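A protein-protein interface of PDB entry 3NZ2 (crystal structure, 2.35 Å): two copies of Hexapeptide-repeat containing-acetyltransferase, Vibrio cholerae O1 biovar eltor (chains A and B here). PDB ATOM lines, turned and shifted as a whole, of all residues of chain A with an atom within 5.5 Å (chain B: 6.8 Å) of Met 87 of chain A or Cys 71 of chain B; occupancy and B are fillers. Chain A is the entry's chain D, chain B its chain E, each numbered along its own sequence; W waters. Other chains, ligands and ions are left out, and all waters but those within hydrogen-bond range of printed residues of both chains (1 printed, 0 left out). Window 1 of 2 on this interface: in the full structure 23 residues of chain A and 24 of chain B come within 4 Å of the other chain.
NE2 of Gln 110 of chain B lies within hydrogen-bond range of OG of Ser 108 of chain A (2.9 Å).
1 position is printed for both chains. Of the 9 pairs that touch across the chains among the printed residues, none has its exchanged pair printed and touching as well.
O of Pro 68 of chain A is in hydrogen-bond range of N of Asn 88 of chain A (2.7 Å). The side-chain carboxylate of Asp 93 of chain B lies close to the side-chain sulfur of Cys 71 of chain B (3.7 Å). O of Cys 71 of chain B sits at hydrogen-bond distance from NZ of Lys 36 of chain B. N of His 70 of chain B lies within hydrogen-bond range of O of Val 89 of chain B, at 2.8 Å. The backbone NH (N) of Met 91 of chain B is in hydrogen-bond range of the backbone carbonyl oxygen (O) of His 70 of chain B. The backbone carbonyl oxygen (O) of Met 87 of chain A lies within hydrogen-bond range of the backbone NH (N) of Ser 108 of chain A, at 3.0 Å.
His 70 of chain B touches Pro 68 of chain A. Asn 86 of chain A touches Leu 92 of chain B. Met 87 of chain A touches Cys 71 of chain B (SD to O, 3.8 Å). CE of Met 87 of chain A touches CD2 of Leu 92 of chain B, at 3.6 Å. Pro 107 of chain A touches Val 90 of chain B. CG of Pro 107 of chain A touches CD1 of Leu 92 of chain B (3.6 Å). Pro 107 of chain A touches Gln 110 of chain B. Val 90 of chain B touches Ser 108 of chain A (CG2 to OG, 3.8 Å).
Hydrophobic or aromatic side chains of chain A that line the printed part of chain B: Pro 68, Met 87 and Pro 107. Of the 20 printed residues of chain B, 5 touch a printed residue of chain A. Hydrophobic or aromatic side chains of chain B that line the printed part of chain A: His 70, Val 90 and Leu 92. Along chain B the printed residues that touch a printed residue of chain A span positions 70 to 110. Among the printed residues, no Asp or Glu carboxylate lies within 4 Å of a Lys or Arg side-chain nitrogen of the other chain.
Met 87 of chain A touches just these residues of chain B: Cys 71 (3.8 Å) and Leu 92 (3.6 Å). Of chain A, only Met 87 (3.8 Å) comes within 4 Å of Cys 71 of chain B. Of the printed residues of chain A, Leu 92 of chain B touches Asn 86, Met 87 and Pro 107. Of the printed residues of chain B, Ser 108 of chain A touches Val 90 and Gln 110. Printed residues of chain B within 4 Å of Pro 68 of chain A: His 70. Of the printed residues of chain A, Val 90 of chain B touches Pro 107 (3.9 Å) and Ser 108 (3.8 Å). Printed residues of chain B within 4 Å of Asn 86 of chain A: Leu 92. Asn 88 of chain A touches none of the printed residues of chain B. The nearest residue of chain B that does not touch Met 87 of chain A is His 70 of chain B (4.1 Å).
Water W1 lies within hydrogen-bond range of the side-chain amide oxygen (OE1) of Gln 110 of chain B, the side-chain amide nitrogen (ND2) of Asn 88 of chain A and the side-chain hydroxyl (OG) of Ser 108 of chain A.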
ATOM      1  N   GLN A  66     -11.741 -27.890   7.388  1.00  0.00           N
ATOM      2  CA  GLN A  66     -13.181 -28.030   7.527  1.00  0.00           C
ATOM      3  C   GLN A  66     -13.885 -26.782   7.072  1.00  0.00           C
ATOM      4  O   GLN A  66     -13.499 -25.692   7.438  1.00  0.00           O
ATOM      5  CB  GLN A  66     -13.586 -28.275   8.992  1.00  0.00           C
ATOM      6  CG  GLN A  66     -13.056 -29.526   9.600  1.00  0.00           C
ATOM      7  CD  GLN A  66     -13.258 -30.701   8.709  1.00  0.00           C
ATOM      8  OE1 GLN A  66     -14.357 -31.216   8.589  1.00  0.00           O
ATOM      9  NE2 GLN A  66     -12.195 -31.121   8.042  1.00  0.00           N
ATOM     10  N   PRO A  67     -14.936 -26.951   6.283  1.00  0.00           N
ATOM     11  CA  PRO A  67     -15.864 -25.897   5.849  1.00  0.00           C
ATOM     12  C   PRO A  67     -16.645 -25.393   7.039  1.00  0.00           C
ATOM     13  O   PRO A  67     -17.042 -26.203   7.853  1.00  0.00           O
ATOM     14  CB  PRO A  67     -16.824 -26.626   4.915  1.00  0.00           C
ATOM     15  CG  PRO A  67     -16.096 -27.880   4.500  1.00  0.00           C
ATOM     16  CD  PRO A  67     -15.115 -28.221   5.562  1.00  0.00           C
ATOM     17  N   PRO A  68     -16.904 -24.076   7.123  1.00  0.00           N
ATOM     18  CA  PRO A  68     -16.500 -23.126   6.097  1.00  0.00           C
ATOM     19  C   PRO A  68     -15.103 -22.622   6.350  1.00  0.00           C
ATOM     20  O   PRO A  68     -14.652 -22.593   7.492  1.00  0.00           O
ATOM     21  CB  PRO A  68     -17.509 -21.985   6.269  1.00  0.00           C
ATOM     22  CG  PRO A  68     -17.864 -22.015   7.642  1.00  0.00           C
ATOM     23  CD  PRO A  68     -17.802 -23.453   8.110  1.00  0.00           C
ATOM     24  N   ILE A  85      -7.335 -28.466  10.231  1.00  0.00           N
ATOM     25  CA  ILE A  85      -7.784 -27.106  10.511  1.00  0.00           C
ATOM     26  C   ILE A  85      -9.278 -27.147  10.766  1.00  0.00           C
ATOM     27  O   ILE A  85     -10.015 -27.684   9.959  1.00  0.00           O
ATOM     28  CB  ILE A  85      -7.501 -26.167   9.317  1.00  0.00           C
ATOM     29  CG1 ILE A  85      -6.005 -26.160   8.990  1.00  0.00           C
ATOM     30  CG2 ILE A  85      -8.076 -24.747   9.592  1.00  0.00           C
ATOM     31  CD1 ILE A  85      -5.620 -25.185   7.917  1.00  0.00           C
ATOM     32  N   ASN A  86      -9.745 -26.604  11.879  1.00  0.00           N
ATOM     33  CA  ASN A  86     -11.178 -26.681  12.114  1.00  0.00           C
ATOM     34  C   ASN A  86     -11.972 -25.614  11.391  1.00  0.00           C
ATOM     35  O   ASN A  86     -11.424 -24.799  10.658  1.00  0.00           O
ATOM     36  CB  ASN A  86     -11.520 -26.708  13.600  1.00  0.00           C
ATOM     37  CG  ASN A  86     -12.600 -27.736  13.932  1.00  0.00           C
ATOM     38  OD1 ASN A  86     -13.628 -27.844  13.240  1.00  0.00           O
ATOM     39  ND2 ASN A  86     -12.358 -28.520  14.986  1.00  0.00           N
ATOM     40  N   MET A  87     -13.282 -25.669  11.591  1.00  0.00           N
ATOM     41  CA  MET A  87     -14.267 -24.792  10.980  1.00  0.00           C
ATOM     42  C   MET A  87     -14.107 -23.290  11.191  1.00  0.00           C
ATOM     43  O   MET A  87     -13.625 -22.831  12.223  1.00  0.00           O
ATOM     44  CB  MET A  87     -15.656 -25.179  11.494  1.00  0.00           C
ATOM     45  CG  MET A  87     -16.166 -26.521  10.999  1.00  0.00           C
ATOM     46  SD  MET A  87     -17.874 -27.041  11.817  1.00  0.00           S
ATOM     47  CE  MET A  87     -17.240 -27.456  13.638  1.00  0.00           C
ATOM     48  N   ASN A  88     -14.579 -22.533  10.206  1.00  0.00           N
ATOM     49  CA  ASN A  88     -14.804 -21.106  10.353  1.00  0.00           C
ATOM     50  C   ASN A  88     -13.532 -20.278  10.530  1.00  0.00           C
ATOM     51  O   ASN A  88     -13.563 -19.177  11.081  1.00  0.00           O
ATOM     52  CB  ASN A  88     -15.810 -20.828  11.463  1.00  0.00           C
ATOM     53  CG  ASN A  88     -16.631 -19.613  11.171  1.00  0.00           C
ATOM     54  OD1 ASN A  88     -16.706 -19.204  10.028  1.00  0.00           O
ATOM     55  ND2 ASN A  88     -17.233 -19.014  12.188  1.00  0.00           N
ATOM     56  N   VAL A  89     -12.421 -20.802  10.025  1.00  0.00           N
ATOM     57  CA  VAL A  89     -11.146 -20.117  10.137  1.00  0.00           C
ATOM     58  C   VAL A  89     -11.025 -18.954   9.160  1.00  0.00           C
ATOM     59  O   VAL A  89     -11.419 -19.055   7.977  1.00  0.00           O
ATOM     60  CB  VAL A  89      -9.983 -21.099   9.947  1.00  0.00           C
ATOM     61  CG1 VAL A  89      -8.683 -20.373   9.660  1.00  0.00           C
ATOM     62  CG2 VAL A  89      -9.842 -21.991  11.199  1.00  0.00           C
ATOM     63  N   GLY A 106      -7.787 -24.851  15.865  1.00  0.00           N
ATOM     64  CA  GLY A 106      -9.176 -24.938  16.281  1.00  0.00           C
ATOM     65  C   GLY A 106     -10.051 -23.900  15.633  1.00  0.00           C
ATOM     66  O   GLY A 106      -9.568 -23.014  14.936  1.00  0.00           O
ATOM     67  N   PRO A 107     -11.360 -24.008  15.856  1.00  0.00           N
ATOM     68  CA  PRO A 107     -12.365 -23.189  15.164  1.00  0.00           C
ATOM     69  C   PRO A 107     -12.199 -21.695  15.371  1.00  0.00           C
ATOM     70  O   PRO A 107     -11.936 -21.226  16.496  1.00  0.00           O
ATOM     71  CB  PRO A 107     -13.662 -23.601  15.846  1.00  0.00           C
ATOM     72  CG  PRO A 107     -13.400 -24.978  16.347  1.00  0.00           C
ATOM     73  CD  PRO A 107     -11.972 -24.988  16.768  1.00  0.00           C
ATOM     74  N   SER A 108     -12.377 -20.964  14.279  1.00  0.00           N
ATOM     75  CA  SER A 108     -12.594 -19.537  14.315  1.00  0.00           C
ATOM     76  C   SER A 108     -11.301 -18.771  14.584  1.00  0.00           C
ATOM     77  O   SER A 108     -11.306 -17.593  14.948  1.00  0.00           O
ATOM     78  CB  SER A 108     -13.720 -19.189  15.314  1.00  0.00           C
ATOM     79  OG  SER A 108     -14.961 -19.783  14.911  1.00  0.00           O
ATOM     80  N   THR A 109     -10.181 -19.453  14.380  1.00  0.00           N
ATOM     81  CA  THR A 109      -8.900 -18.811  14.529  1.00  0.00           C
ATOM     82  C   THR A 109      -8.659 -17.858  13.363  1.00  0.00           C
ATOM     83  O   THR A 109      -9.208 -18.038  12.284  1.00  0.00           O
ATOM     84  CB  THR A 109      -7.796 -19.852  14.670  1.00  0.00           C
ATOM     85  OG1 THR A 109      -7.884 -20.400  15.987  1.00  0.00           O
ATOM     86  CG2 THR A 109      -6.401 -19.207  14.520  1.00  0.00           C
ATOM     87  N   ARG B  29     -21.379 -37.674  10.839  1.00  0.00           N
ATOM     88  CA  ARG B  29     -20.744 -36.452  10.373  1.00  0.00           C
ATOM     89  C   ARG B  29     -21.316 -35.947   9.033  1.00  0.00           C
ATOM     90  O   ARG B  29     -21.484 -34.746   8.828  1.00  0.00           O
ATOM     91  CB  ARG B  29     -19.243 -36.698  10.266  1.00  0.00           C
ATOM     92  CG  ARG B  29     -18.387 -35.501  10.519  1.00  0.00           C
ATOM     93  CD  ARG B  29     -16.953 -35.909  10.345  1.00  0.00           C
ATOM     94  NE  ARG B  29     -16.238 -36.093  11.601  1.00  0.00           N
ATOM     95  CZ  ARG B  29     -15.616 -37.214  11.966  1.00  0.00           C
ATOM     96  NH1 ARG B  29     -15.628 -38.294  11.184  1.00  0.00           N
ATOM     97  NH2 ARG B  29     -14.988 -37.258  13.138  1.00  0.00           N
ATOM     98  N   ALA B  32     -24.866 -34.705   9.477  1.00  0.00           N
ATOM     99  CA  ALA B  32     -24.698 -33.363  10.012  1.00  0.00           C
ATOM    100  C   ALA B  32     -24.308 -32.303   8.955  1.00  0.00           C
ATOM    101  O   ALA B  32     -24.931 -31.254   8.873  1.00  0.00           O
ATOM    102  CB  ALA B  32     -23.729 -33.389  11.147  1.00  0.00           C
ATOM    103  N   GLY B  33     -23.294 -32.600   8.145  1.00  0.00           N
ATOM    104  CA  GLY B  33     -22.904 -31.769   7.006  1.00  0.00           C
ATOM    105  C   GLY B  33     -24.067 -31.414   6.097  1.00  0.00           C
ATOM    106  O   GLY B  33     -24.310 -30.229   5.818  1.00  0.00           O
ATOM    107  N   LYS B  36     -26.638 -29.094   7.907  1.00  0.00           N
ATOM    108  CA  LYS B  36     -26.177 -27.738   8.164  1.00  0.00           C
ATOM    109  C   LYS B  36     -26.393 -26.911   6.904  1.00  0.00           C
ATOM    110  O   LYS B  36     -26.895 -25.771   6.936  1.00  0.00           O
ATOM    111  CB  LYS B  36     -24.704 -27.741   8.571  1.00  0.00           C
ATOM    112  CG  LYS B  36     -24.479 -28.055  10.037  1.00  0.00           C
ATOM    113  CD  LYS B  36     -23.164 -28.802  10.300  1.00  0.00           C
ATOM    114  CE  LYS B  36     -22.017 -28.304   9.435  1.00  0.00           C
ATOM    115  NZ  LYS B  36     -20.787 -29.110   9.667  1.00  0.00           N
ATOM    116  N   LEU B  55     -31.528 -32.558  12.899  1.00  0.00           N
ATOM    117  CA  LEU B  55     -30.118 -32.328  13.146  1.00  0.00           C
ATOM    118  C   LEU B  55     -29.793 -32.519  14.651  1.00  0.00           C
ATOM    119  O   LEU B  55     -28.858 -33.257  15.010  1.00  0.00           O
ATOM    120  CB  LEU B  55     -29.699 -30.930  12.633  1.00  0.00           C
ATOM    121  CG  LEU B  55     -28.339 -30.491  13.186  1.00  0.00           C
ATOM    122  CD1 LEU B  55     -27.214 -31.280  12.484  1.00  0.00           C
ATOM    123  CD2 LEU B  55     -28.143 -29.004  13.044  1.00  0.00           C
ATOM    124  N   PHE B  56     -30.566 -31.853  15.514  1.00  0.00           N
ATOM    125  CA  PHE B  56     -30.280 -31.821  16.950  1.00  0.00           C
ATOM    126  C   PHE B  56     -30.866 -33.034  17.664  1.00  0.00           C
ATOM    127  O   PHE B  56     -31.787 -33.667  17.130  1.00  0.00           O
ATOM    128  CB  PHE B  56     -30.841 -30.537  17.593  1.00  0.00           C
ATOM    129  CG  PHE B  56     -30.186 -29.284  17.109  1.00  0.00           C
ATOM    130  CD1 PHE B  56     -28.814 -29.243  16.887  1.00  0.00           C
ATOM    131  CD2 PHE B  56     -30.936 -28.148  16.856  1.00  0.00           C
ATOM    132  CE1 PHE B  56     -28.212 -28.094  16.416  1.00  0.00           C
ATOM    133  CE2 PHE B  56     -30.321 -26.968  16.406  1.00  0.00           C
ATOM    134  CZ  PHE B  56     -28.970 -26.944  16.178  1.00  0.00           C
ATOM    135  N   PHE B  69     -25.322 -21.674  11.513  1.00  0.00           N
ATOM    136  CA  PHE B  69     -24.990 -22.424  12.706  1.00  0.00           C
ATOM    137  C   PHE B  69     -24.058 -23.557  12.316  1.00  0.00           C
ATOM    138  O   PHE B  69     -24.295 -24.256  11.358  1.00  0.00           O
ATOM    139  CB  PHE B  69     -26.238 -22.964  13.390  1.00  0.00           C
ATOM    140  CG  PHE B  69     -25.950 -23.863  14.553  1.00  0.00           C
ATOM    141  CD1 PHE B  69     -25.810 -23.352  15.816  1.00  0.00           C
ATOM    142  CD2 PHE B  69     -25.811 -25.223  14.378  1.00  0.00           C
ATOM    143  CE1 PHE B  69     -25.546 -24.171  16.862  1.00  0.00           C
ATOM    144  CE2 PHE B  69     -25.542 -26.037  15.430  1.00  0.00           C
ATOM    145  CZ  PHE B  69     -25.414 -25.513  16.668  1.00  0.00           C
ATOM    146  N   HIS B  70     -22.987 -23.728  13.067  1.00  0.00           N
ATOM    147  CA  HIS B  70     -22.013 -24.778  12.800  1.00  0.00           C
ATOM    148  C   HIS B  70     -21.807 -25.756  13.937  1.00  0.00           C
ATOM    149  O   HIS B  70     -21.712 -25.379  15.087  1.00  0.00           O
ATOM    150  CB  HIS B  70     -20.681 -24.172  12.413  1.00  0.00           C
ATOM    151  CG  HIS B  70     -20.801 -23.096  11.398  1.00  0.00           C
ATOM    152  ND1 HIS B  70     -21.120 -23.355  10.088  1.00  0.00           N
ATOM    153  CD2 HIS B  70     -20.694 -21.757  11.504  1.00  0.00           C
ATOM    154  CE1 HIS B  70     -21.183 -22.220   9.425  1.00  0.00           C
ATOM    155  NE2 HIS B  70     -20.928 -21.237  10.262  1.00  0.00           N
ATOM    156  N   CYS B  71     -21.741 -27.023  13.583  1.00  0.00           N
ATOM    157  CA  CYS B  71     -21.536 -28.095  14.531  1.00  0.00           C
ATOM    158  C   CYS B  71     -20.912 -29.278  13.812  1.00  0.00           C
ATOM    159  O   CYS B  71     -20.829 -29.307  12.602  1.00  0.00           O
ATOM    160  CB  CYS B  71     -22.834 -28.483  15.230  1.00  0.00           C
ATOM    161  SG  CYS B  71     -24.004 -29.306  14.226  1.00  0.00           S
ATOM    162  N   GLU B  72     -20.421 -30.234  14.568  1.00  0.00           N
ATOM    163  CA  GLU B  72     -19.806 -31.389  13.965  1.00  0.00           C
ATOM    164  C   GLU B  72     -20.711 -32.608  13.825  1.00  0.00           C
ATOM    165  O   GLU B  72     -20.690 -33.277  12.811  1.00  0.00           O
ATOM    166  CB  GLU B  72     -18.559 -31.751  14.740  1.00  0.00           C
ATOM    167  CG  GLU B  72     -17.695 -32.705  14.042  1.00  0.00           C
ATOM    168  CD  GLU B  72     -16.454 -32.958  14.811  1.00  0.00           C
ATOM    169  OE1 GLU B  72     -16.294 -32.291  15.845  1.00  0.00           O
ATOM    170  OE2 GLU B  72     -15.647 -33.812  14.395  1.00  0.00           O
ATOM    171  N   PHE B  73     -21.481 -32.907  14.861  1.00  0.00           N
ATOM    172  CA  PHE B  73     -22.342 -34.072  14.836  1.00  0.00           C
ATOM    173  C   PHE B  73     -23.816 -33.766  14.994  1.00  0.00           C
ATOM    174  O   PHE B  73     -24.642 -34.400  14.368  1.00  0.00           O
ATOM    175  CB  PHE B  73     -21.884 -35.089  15.878  1.00  0.00           C
ATOM    176  CG  PHE B  73     -20.434 -35.438  15.782  1.00  0.00           C
ATOM    177  CD1 PHE B  73     -19.998 -36.412  14.917  1.00  0.00           C
ATOM    178  CD2 PHE B  73     -19.501 -34.795  16.559  1.00  0.00           C
ATOM    179  CE1 PHE B  73     -18.677 -36.723  14.839  1.00  0.00           C
ATOM    180  CE2 PHE B  73     -18.193 -35.112  16.471  1.00  0.00           C
ATOM    181  CZ  PHE B  73     -17.781 -36.074  15.615  1.00  0.00           C
ATOM    182  N   GLY B  74     -24.146 -32.782  15.815  1.00  0.00           N
ATOM    183  CA  GLY B  74     -25.526 -32.414  16.027  1.00  0.00           C
ATOM    184  C   GLY B  74     -26.421 -33.239  16.935  1.00  0.00           C
ATOM    185  O   GLY B  74     -27.170 -32.676  17.715  1.00  0.00           O
ATOM    186  N   LYS B  75     -26.388 -34.563  16.816  1.00  0.00           N
ATOM    187  CA  LYS B  75     -27.349 -35.379  17.547  1.00  0.00           C
ATOM    188  C   LYS B  75     -27.065 -35.357  19.051  1.00  0.00           C
ATOM    189  O   LYS B  75     -27.932 -35.678  19.865  1.00  0.00           O
ATOM    190  CB  LYS B  75     -27.383 -36.814  17.033  1.00  0.00           C
ATOM    191  CG  LYS B  75     -28.532 -37.122  16.077  1.00  0.00           C
ATOM    192  CD  LYS B  75     -29.977 -36.806  16.593  1.00  0.00           C
ATOM    193  CE  LYS B  75     -30.896 -36.813  15.359  1.00  0.00           C
ATOM    194  NZ  LYS B  75     -32.265 -36.250  15.436  1.00  0.00           N
ATOM    195  N   ILE B  77     -26.515 -32.683  20.700  1.00  0.00           N
ATOM    196  CA  ILE B  77     -26.939 -31.382  21.209  1.00  0.00           C
ATOM    197  C   ILE B  77     -28.406 -31.352  21.626  1.00  0.00           C
ATOM    198  O   ILE B  77     -29.298 -31.753  20.876  1.00  0.00           O
ATOM    199  CB  ILE B  77     -26.717 -30.278  20.128  1.00  0.00           C
ATOM    200  CG1 ILE B  77     -25.224 -30.082  19.813  1.00  0.00           C
ATOM    201  CG2 ILE B  77     -27.417 -28.955  20.512  1.00  0.00           C
ATOM    202  CD1 ILE B  77     -24.976 -29.092  18.726  1.00  0.00           C
ATOM    203  N   VAL B  89     -22.727 -19.404  15.495  1.00  0.00           N
ATOM    204  CA  VAL B  89     -22.261 -20.226  16.607  1.00  0.00           C
ATOM    205  C   VAL B  89     -21.566 -21.477  16.118  1.00  0.00           C
ATOM    206  O   VAL B  89     -22.028 -22.106  15.176  1.00  0.00           O
ATOM    207  CB  VAL B  89     -23.424 -20.640  17.468  1.00  0.00           C
ATOM    208  CG1 VAL B  89     -23.012 -21.715  18.471  1.00  0.00           C
ATOM    209  CG2 VAL B  89     -23.970 -19.408  18.119  1.00  0.00           C
ATOM    210  N   VAL B  90     -20.444 -21.807  16.750  1.00  0.00           N
ATOM    211  CA  VAL B  90     -19.716 -23.032  16.469  1.00  0.00           C
ATOM    212  C   VAL B  90     -19.717 -23.939  17.699  1.00  0.00           C
ATOM    213  O   VAL B  90     -19.264 -23.527  18.793  1.00  0.00           O
ATOM    214  CB  VAL B  90     -18.261 -22.743  16.158  1.00  0.00           C
ATOM    215  CG1 VAL B  90     -17.501 -24.029  15.942  1.00  0.00           C
ATOM    216  CG2 VAL B  90     -18.141 -21.851  14.964  1.00  0.00           C
ATOM    217  N   MET B  91     -20.189 -25.177  17.518  1.00  0.00           N
ATOM    218  CA  MET B  91     -20.114 -26.188  18.575  1.00  0.00           C
ATOM    219  C   MET B  91     -19.369 -27.423  18.137  1.00  0.00           C
ATOM    220  O   MET B  91     -19.789 -28.112  17.195  1.00  0.00           O
ATOM    221  CB  MET B  91     -21.504 -26.604  19.021  1.00  0.00           C
ATOM    222  CG  MET B  91     -22.365 -25.435  19.438  1.00  0.00           C
ATOM    223  SD  MET B  91     -23.972 -26.092  20.297  1.00  0.00           S
ATOM    224  CE  MET B  91     -24.649 -24.446  21.117  1.00  0.00           C
ATOM    225  N   LEU B  92     -18.264 -27.700  18.821  1.00  0.00           N
ATOM    226  CA  LEU B  92     -17.577 -28.978  18.704  1.00  0.00           C
ATOM    227  C   LEU B  92     -18.276 -29.916  19.665  1.00  0.00           C
ATOM    228  O   LEU B  92     -18.099 -29.841  20.890  1.00  0.00           O
ATOM    229  CB  LEU B  92     -16.111 -28.828  19.077  1.00  0.00           C
ATOM    230  CG  LEU B  92     -15.354 -27.918  18.110  1.00  0.00           C
ATOM    231  CD1 LEU B  92     -13.884 -27.860  18.464  1.00  0.00           C
ATOM    232  CD2 LEU B  92     -15.573 -28.433  16.676  1.00  0.00           C
ATOM    233  N   ASP B  93     -19.084 -30.792  19.098  1.00  0.00           N
ATOM    234  CA  ASP B  93     -20.046 -31.556  19.858  1.00  0.00           C
ATOM    235  C   ASP B  93     -19.790 -33.071  19.884  1.00  0.00           C
ATOM    236  O   ASP B  93     -20.733 -33.855  19.847  1.00  0.00           O
ATOM    237  CB  ASP B  93     -21.474 -31.235  19.351  1.00  0.00           C
ATOM    238  CG  ASP B  93     -21.615 -31.305  17.807  1.00  0.00           C
ATOM    239  OD1 ASP B  93     -20.641 -31.687  17.093  1.00  0.00           O
ATOM    240  OD2 ASP B  93     -22.733 -30.982  17.306  1.00  0.00           O
ATOM    241  N   GLN B 110     -18.564 -20.020  21.007  1.00  0.00           N
ATOM    242  CA  GLN B 110     -18.017 -21.334  20.747  1.00  0.00           C
ATOM    243  C   GLN B 110     -18.106 -22.331  21.879  1.00  0.00           C
ATOM    244  O   GLN B 110     -17.724 -22.057  22.988  1.00  0.00           O
ATOM    245  CB  GLN B 110     -16.555 -21.197  20.349  1.00  0.00           C
ATOM    246  CG  GLN B 110     -16.215 -19.928  19.635  1.00  0.00           C
ATOM    247  CD  GLN B 110     -16.270 -20.078  18.145  1.00  0.00           C
ATOM    248  OE1 GLN B 110     -17.110 -19.492  17.492  1.00  0.00           O
ATOM    249  NE2 GLN B 110     -15.374 -20.862  17.603  1.00  0.00           N
HETATM  250  O   HOH W   1     -17.771 -18.486  15.052  1.00  0.00           O
